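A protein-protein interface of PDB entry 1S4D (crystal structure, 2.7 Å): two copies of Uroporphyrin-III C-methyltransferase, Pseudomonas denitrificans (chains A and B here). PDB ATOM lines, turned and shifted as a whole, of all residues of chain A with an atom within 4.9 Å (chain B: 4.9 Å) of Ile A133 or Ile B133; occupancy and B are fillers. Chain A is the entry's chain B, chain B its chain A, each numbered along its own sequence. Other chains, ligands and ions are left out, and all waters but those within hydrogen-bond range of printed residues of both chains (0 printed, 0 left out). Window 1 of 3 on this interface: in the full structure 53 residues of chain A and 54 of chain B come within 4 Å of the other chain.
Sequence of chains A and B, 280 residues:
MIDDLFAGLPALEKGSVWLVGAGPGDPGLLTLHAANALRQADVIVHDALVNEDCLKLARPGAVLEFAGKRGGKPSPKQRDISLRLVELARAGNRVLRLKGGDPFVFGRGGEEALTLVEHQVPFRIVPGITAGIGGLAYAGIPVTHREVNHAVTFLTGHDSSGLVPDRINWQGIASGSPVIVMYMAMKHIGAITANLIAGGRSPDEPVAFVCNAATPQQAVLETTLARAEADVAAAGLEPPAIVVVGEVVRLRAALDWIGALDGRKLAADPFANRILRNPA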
ATOM      1  N   ASP A 102      35.773  -9.179  20.515  1.00  0.00           N
ATOM      2  CA  ASP A 102      35.750 -10.026  21.705  1.00  0.00           C
ATOM      3  C   ASP A 102      36.849 -11.093  21.608  1.00  0.00           C
ATOM      4  O   ASP A 102      37.017 -11.730  20.575  1.00  0.00           O
ATOM      5  CB  ASP A 102      34.402 -10.729  21.832  1.00  0.00           C
ATOM      6  CG  ASP A 102      34.300 -11.529  23.092  1.00  0.00           C
ATOM      7  OD1 ASP A 102      34.402 -12.780  23.036  1.00  0.00           O
ATOM      8  OD2 ASP A 102      34.146 -10.983  24.199  1.00  0.00           O
ATOM      9  N   VAL A 105      35.471 -14.650  20.255  1.00  0.00           N
ATOM     10  CA  VAL A 105      34.762 -14.820  18.987  1.00  0.00           C
ATOM     11  C   VAL A 105      35.767 -14.861  17.824  1.00  0.00           C
ATOM     12  O   VAL A 105      36.270 -13.834  17.413  1.00  0.00           O
ATOM     13  CB  VAL A 105      33.650 -13.745  18.819  1.00  0.00           C
ATOM     14  CG1 VAL A 105      32.820 -13.954  17.531  1.00  0.00           C
ATOM     15  CG2 VAL A 105      32.744 -13.737  20.051  1.00  0.00           C
ATOM     16  N   THR A 130      31.481  -7.442  19.801  1.00  0.00           N
ATOM     17  CA  THR A 130      31.903  -8.207  18.617  1.00  0.00           C
ATOM     18  C   THR A 130      31.419  -7.580  17.302  1.00  0.00           C
ATOM     19  O   THR A 130      30.325  -7.006  17.214  1.00  0.00           O
ATOM     20  CB  THR A 130      31.513  -9.733  18.759  1.00  0.00           C
ATOM     21  OG1 THR A 130      32.148 -10.497  17.718  1.00  0.00           O
ATOM     22  CG2 THR A 130      30.041  -9.982  18.498  1.00  0.00           C
ATOM     23  N   ALA A 131      32.223  -7.706  16.268  1.00  0.00           N
ATOM     24  CA  ALA A 131      31.876  -7.068  14.999  1.00  0.00           C
ATOM     25  C   ALA A 131      30.502  -7.555  14.491  1.00  0.00           C
ATOM     26  O   ALA A 131      29.711  -6.745  14.000  1.00  0.00           O
ATOM     27  CB  ALA A 131      32.965  -7.286  13.964  1.00  0.00           C
ATOM     28  N   GLY A 132      30.227  -8.861  14.639  1.00  0.00           N
ATOM     29  CA  GLY A 132      28.980  -9.452  14.194  1.00  0.00           C
ATOM     30  C   GLY A 132      27.718  -9.025  14.934  1.00  0.00           C
ATOM     31  O   GLY A 132      26.618  -9.256  14.427  1.00  0.00           O
ATOM     32  N   ILE A 133      27.835  -8.427  16.123  1.00  0.00           N
ATOM     33  CA  ILE A 133      26.646  -7.902  16.788  1.00  0.00           C
ATOM     34  C   ILE A 133      26.715  -6.396  16.848  1.00  0.00           C
ATOM     35  O   ILE A 133      25.843  -5.709  16.299  1.00  0.00           O
ATOM     36  CB  ILE A 133      26.428  -8.502  18.190  1.00  0.00           C
ATOM     37  CG1 ILE A 133      26.324 -10.031  18.105  1.00  0.00           C
ATOM     38  CG2 ILE A 133      25.182  -7.930  18.814  1.00  0.00           C
ATOM     39  CD1 ILE A 133      26.538 -10.759  19.437  1.00  0.00           C
ATOM     40  N   GLY A 134      27.757  -5.864  17.473  1.00  0.00           N
ATOM     41  CA  GLY A 134      27.848  -4.422  17.633  1.00  0.00           C
ATOM     42  C   GLY A 134      28.134  -3.730  16.320  1.00  0.00           C
ATOM     43  O   GLY A 134      27.500  -2.728  16.005  1.00  0.00           O
ATOM     44  N   GLY A 135      29.089  -4.271  15.557  1.00  0.00           N
ATOM     45  CA  GLY A 135      29.375  -3.801  14.217  1.00  0.00           C
ATOM     46  C   GLY A 135      28.152  -3.666  13.341  1.00  0.00           C
ATOM     47  O   GLY A 135      27.933  -2.619  12.724  1.00  0.00           O
ATOM     48  N   LEU A 136      27.326  -4.704  13.307  1.00  0.00           N
ATOM     49  CA  LEU A 136      26.133  -4.662  12.477  1.00  0.00           C
ATOM     50  C   LEU A 136      25.113  -3.637  12.978  1.00  0.00           C
ATOM     51  O   LEU A 136      24.441  -2.976  12.169  1.00  0.00           O
ATOM     52  CB  LEU A 136      25.528  -6.059  12.316  1.00  0.00           C
ATOM     53  CG  LEU A 136      26.425  -7.022  11.521  1.00  0.00           C
ATOM     54  CD1 LEU A 136      25.813  -8.370  11.547  1.00  0.00           C
ATOM     55  CD2 LEU A 136      26.589  -6.597  10.086  1.00  0.00           C
ATOM     56  N   ALA A 137      25.036  -3.480  14.306  1.00  0.00           N
ATOM     57  CA  ALA A 137      24.266  -2.389  14.904  1.00  0.00           C
ATOM     58  C   ALA A 137      24.648  -1.027  14.326  1.00  0.00           C
ATOM     59  O   ALA A 137      23.766  -0.172  14.096  1.00  0.00           O
ATOM     60  CB  ALA A 137      24.416  -2.380  16.405  1.00  0.00           C
ATOM     61  N   VAL A 143      20.882  -8.225  14.575  1.00  0.00           N
ATOM     62  CA  VAL A 143      21.261  -9.592  14.330  1.00  0.00           C
ATOM     63  C   VAL A 143      20.080 -10.556  14.643  1.00  0.00           C
ATOM     64  O   VAL A 143      20.060 -11.726  14.265  1.00  0.00           O
ATOM     65  CB  VAL A 143      22.555  -9.804  15.159  1.00  0.00           C
ATOM     66  CG1 VAL A 143      22.326 -10.552  16.465  1.00  0.00           C
ATOM     67  CG2 VAL A 143      23.663 -10.348  14.307  1.00  0.00           C
ATOM     68  N   PHE A 154      26.756 -17.610  13.657  1.00  0.00           N
ATOM     69  CA  PHE A 154      27.985 -16.879  13.350  1.00  0.00           C
ATOM     70  C   PHE A 154      28.962 -17.880  12.749  1.00  0.00           C
ATOM     71  O   PHE A 154      28.980 -19.025  13.191  1.00  0.00           O
ATOM     72  CB  PHE A 154      28.575 -16.290  14.622  1.00  0.00           C
ATOM     73  CG  PHE A 154      27.860 -15.077  15.140  1.00  0.00           C
ATOM     74  CD1 PHE A 154      28.536 -14.140  15.880  1.00  0.00           C
ATOM     75  CD2 PHE A 154      26.509 -14.876  14.919  1.00  0.00           C
ATOM     76  CE1 PHE A 154      27.856 -13.016  16.377  1.00  0.00           C
ATOM     77  CE2 PHE A 154      25.831 -13.758  15.410  1.00  0.00           C
ATOM     78  CZ  PHE A 154      26.480 -12.841  16.116  1.00  0.00           C
ATOM     79  N   TYR A 183      32.238 -14.015   9.536  1.00  0.00           N
ATOM     80  CA  TYR A 183      33.536 -13.427   9.837  1.00  0.00           C
ATOM     81  C   TYR A 183      34.539 -13.974   8.826  1.00  0.00           C
ATOM     82  O   TYR A 183      34.389 -15.104   8.369  1.00  0.00           O
ATOM     83  CB  TYR A 183      33.986 -13.864  11.237  1.00  0.00           C
ATOM     84  CG  TYR A 183      33.238 -13.210  12.390  1.00  0.00           C
ATOM     85  CD1 TYR A 183      31.950 -13.652  12.786  1.00  0.00           C
ATOM     86  CD2 TYR A 183      33.824 -12.176  13.107  1.00  0.00           C
ATOM     87  CE1 TYR A 183      31.265 -13.046  13.845  1.00  0.00           C
ATOM     88  CE2 TYR A 183      33.163 -11.581  14.153  1.00  0.00           C
ATOM     89  CZ  TYR A 183      31.888 -12.005  14.512  1.00  0.00           C
ATOM     90  OH  TYR A 183      31.274 -11.356  15.554  1.00  0.00           O
ATOM     91  N   ASP B 102      22.737  -6.866  25.254  1.00  0.00           N
ATOM     92  CA  ASP B 102      22.856  -6.038  24.075  1.00  0.00           C
ATOM     93  C   ASP B 102      21.472  -5.790  23.536  1.00  0.00           C
ATOM     94  O   ASP B 102      20.628  -6.688  23.523  1.00  0.00           O
ATOM     95  CB  ASP B 102      23.685  -6.761  23.022  1.00  0.00           C
ATOM     96  CG  ASP B 102      23.615  -6.100  21.684  1.00  0.00           C
ATOM     97  OD1 ASP B 102      24.401  -5.138  21.472  1.00  0.00           O
ATOM     98  OD2 ASP B 102      22.806  -6.471  20.803  1.00  0.00           O
ATOM     99  N   VAL B 105      20.341  -8.418  20.622  1.00  0.00           N
ATOM    100  CA  VAL B 105      20.403  -9.847  20.848  1.00  0.00           C
ATOM    101  C   VAL B 105      19.220 -10.247  21.739  1.00  0.00           C
ATOM    102  O   VAL B 105      19.364 -10.420  22.961  1.00  0.00           O
ATOM    103  CB  VAL B 105      21.728 -10.232  21.475  1.00  0.00           C
ATOM    104  CG1 VAL B 105      21.812 -11.747  21.647  1.00  0.00           C
ATOM    105  CG2 VAL B 105      22.852  -9.739  20.612  1.00  0.00           C
ATOM    106  N   THR B 130      26.644  -9.332  25.576  1.00  0.00           N
ATOM    107  CA  THR B 130      25.521 -10.222  25.660  1.00  0.00           C
ATOM    108  C   THR B 130      25.882 -11.421  26.515  1.00  0.00           C
ATOM    109  O   THR B 130      27.028 -11.883  26.507  1.00  0.00           O
ATOM    110  CB  THR B 130      25.056 -10.649  24.234  1.00  0.00           C
ATOM    111  OG1 THR B 130      23.846 -11.411  24.333  1.00  0.00           O
ATOM    112  CG2 THR B 130      26.013 -11.621  23.564  1.00  0.00           C
ATOM    113  N   ALA B 131      24.899 -11.931  27.241  1.00  0.00           N
ATOM    114  CA  ALA B 131      25.082 -13.093  28.110  1.00  0.00           C
ATOM    115  C   ALA B 131      25.614 -14.330  27.383  1.00  0.00           C
ATOM    116  O   ALA B 131      26.403 -15.069  27.961  1.00  0.00           O
ATOM    117  CB  ALA B 131      23.784 -13.420  28.847  1.00  0.00           C
ATOM    118  N   GLY B 132      25.201 -14.530  26.129  1.00  0.00           N
ATOM    119  CA  GLY B 132      25.643 -15.650  25.316  1.00  0.00           C
ATOM    120  C   GLY B 132      27.110 -15.642  24.909  1.00  0.00           C
ATOM    121  O   GLY B 132      27.633 -16.662  24.456  1.00  0.00           O
ATOM    122  N   ILE B 133      27.782 -14.504  25.045  1.00  0.00           N
ATOM    123  CA  ILE B 133      29.226 -14.463  24.786  1.00  0.00           C
ATOM    124  C   ILE B 133      30.044 -14.064  26.020  1.00  0.00           C
ATOM    125  O   ILE B 133      30.921 -14.817  26.466  1.00  0.00           O
ATOM    126  CB  ILE B 133      29.565 -13.580  23.575  1.00  0.00           C
ATOM    127  CG1 ILE B 133      28.796 -14.070  22.351  1.00  0.00           C
ATOM    128  CG2 ILE B 133      31.048 -13.627  23.315  1.00  0.00           C
ATOM    129  CD1 ILE B 133      28.767 -13.073  21.222  1.00  0.00           C
ATOM    130  N   GLY B 134      29.749 -12.903  26.586  1.00  0.00           N
ATOM    131  CA  GLY B 134      30.490 -12.452  27.753  1.00  0.00           C
ATOM    132  C   GLY B 134      30.187 -13.267  28.997  1.00  0.00           C
ATOM    133  O   GLY B 134      31.103 -13.668  29.715  1.00  0.00           O
ATOM    134  N   GLY B 135      28.899 -13.520  29.239  1.00  0.00           N
ATOM    135  CA  GLY B 135      28.472 -14.342  30.350  1.00  0.00           C
ATOM    136  C   GLY B 135      29.188 -15.669  30.298  1.00  0.00           C
ATOM    137  O   GLY B 135      29.916 -16.029  31.234  1.00  0.00           O
ATOM    138  N   LEU B 136      29.042 -16.377  29.184  1.00  0.00           N
ATOM    139  CA  LEU B 136      29.798 -17.613  28.989  1.00  0.00           C
ATOM    140  C   LEU B 136      31.260 -17.451  29.376  1.00  0.00           C
ATOM    141  O   LEU B 136      31.804 -18.319  30.078  1.00  0.00           O
ATOM    142  CB  LEU B 136      29.634 -18.157  27.576  1.00  0.00           C
ATOM    143  CG  LEU B 136      28.200 -18.671  27.414  1.00  0.00           C
ATOM    144  CD1 LEU B 136      28.075 -19.569  26.213  1.00  0.00           C
ATOM    145  CD2 LEU B 136      27.783 -19.404  28.670  1.00  0.00           C
ATOM    146  N   ALA B 137      31.879 -16.330  28.980  1.00  0.00           N
ATOM    147  CA  ALA B 137      33.289 -16.076  29.324  1.00  0.00           C
ATOM    148  C   ALA B 137      33.563 -16.081  30.833  1.00  0.00           C
ATOM    149  O   ALA B 137      34.586 -16.607  31.300  1.00  0.00           O
ATOM    150  CB  ALA B 137      33.752 -14.790  28.725  1.00  0.00           C
ATOM    151  N   VAL B 143      32.721 -19.162  23.210  1.00  0.00           N
ATOM    152  CA  VAL B 143      31.739 -19.591  22.195  1.00  0.00           C
ATOM    153  C   VAL B 143      32.390 -20.150  20.935  1.00  0.00           C
ATOM    154  O   VAL B 143      31.763 -20.883  20.207  1.00  0.00           O
ATOM    155  CB  VAL B 143      30.748 -18.478  21.811  1.00  0.00           C
ATOM    156  CG1 VAL B 143      29.865 -18.123  23.002  1.00  0.00           C
ATOM    157  CG2 VAL B 143      31.472 -17.231  21.310  1.00  0.00           C
ATOM    158  N   PHE B 154      23.056 -18.946  17.963  1.00  0.00           N
ATOM    159  CA  PHE B 154      22.437 -18.355  19.132  1.00  0.00           C
ATOM    160  C   PHE B 154      20.923 -18.420  18.908  1.00  0.00           C
ATOM    161  O   PHE B 154      20.397 -17.983  17.872  1.00  0.00           O
ATOM    162  CB  PHE B 154      22.921 -16.906  19.340  1.00  0.00           C
ATOM    163  CG  PHE B 154      24.408 -16.775  19.480  1.00  0.00           C
ATOM    164  CD1 PHE B 154      25.221 -16.609  18.368  1.00  0.00           C
ATOM    165  CD2 PHE B 154      25.008 -16.814  20.722  1.00  0.00           C
ATOM    166  CE1 PHE B 154      26.609 -16.481  18.519  1.00  0.00           C
ATOM    167  CE2 PHE B 154      26.397 -16.697  20.879  1.00  0.00           C
ATOM    168  CZ  PHE B 154      27.188 -16.539  19.803  1.00  0.00           C
ATOM    169  N   TYR B 183      19.242 -18.911  24.790  1.00  0.00           N
ATOM    170  CA  TYR B 183      18.592 -17.910  25.613  1.00  0.00           C
ATOM    171  C   TYR B 183      17.181 -18.387  25.896  1.00  0.00           C
ATOM    172  O   TYR B 183      16.546 -19.021  25.030  1.00  0.00           O
ATOM    173  CB  TYR B 183      18.495 -16.598  24.823  1.00  0.00           C
ATOM    174  CG  TYR B 183      19.808 -15.897  24.578  1.00  0.00           C
ATOM    175  CD1 TYR B 183      20.698 -16.342  23.595  1.00  0.00           C
ATOM    176  CD2 TYR B 183      20.152 -14.766  25.317  1.00  0.00           C
ATOM    177  CE1 TYR B 183      21.905 -15.669  23.365  1.00  0.00           C
ATOM    178  CE2 TYR B 183      21.334 -14.092  25.088  1.00  0.00           C
ATOM    179  CZ  TYR B 183      22.200 -14.539  24.129  1.00  0.00           C
ATOM    180  OH  TYR B 183      23.382 -13.861  23.962  1.00  0.00           O
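The backbone NH (N) of Val B105 is in hydrogen-bond range of the side-chain carboxylate (OD2) of Asp B102 (3.1 Å).
OD1 of Asp A102 touches CG2 of Ile B133, at 3.5 Å. Val A105 touches Ile B133 (CG2 to CG2, 3.7 Å). Val A105 touches Val B143. CG2 of Ile A133 touches OD2 of Asp B102, 3.4 Å away. Val B105 touches Ile A133. CD1 of Ile A133 touches CD1 of Ile B133 (3.7 Å). Phe B154 touches Phe A154 (CE1 to CG, 3.9 Å).
Ile B133 touches just these residues of chain A: Asp A102 (3.5 Å), Val A105 (3.7 Å) and Ile A133 (3.7 Å). Printed residues of chain B within 4 Å of Val A105: Ile B133 and Val B143. Of the printed residues of chain B, Phe A154 touches Phe B154. Ala A137 touches none of the printed residues of chain B. Gly B135 touches none of the printed residues of chain A.
Of the 13 printed residues of chain A, 4 touch a printed residue of chain B. Hydrophobic or aromatic side chains of chain A that line the printed part of chain B: Val A105, Ile A133 and Phe A154. Among the printed residues, no Asp or Glu carboxylate lies within 4 Å of a Lys or Arg side-chain nitrogen of the other chain.
Asp A102 touches Ile B133, and with the chains exchanged Ile A133 touches Asp B102. Val A105 touches Val B143, but with the chains exchanged Val A143 does not touch Val B105 (4.3 Å). Ile B133 touches its own counterpart, Ile A133. Phe A154 touches its own counterpart, Phe B154. Positions printed for both chains: 102, 105, 130, 131, 132, 133, 134, 135, 136, 137, 143, 154 and 183. Of the 7 pairs that touch across the chains among the printed residues, 6 have their exchanged pair printed and touching as well.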
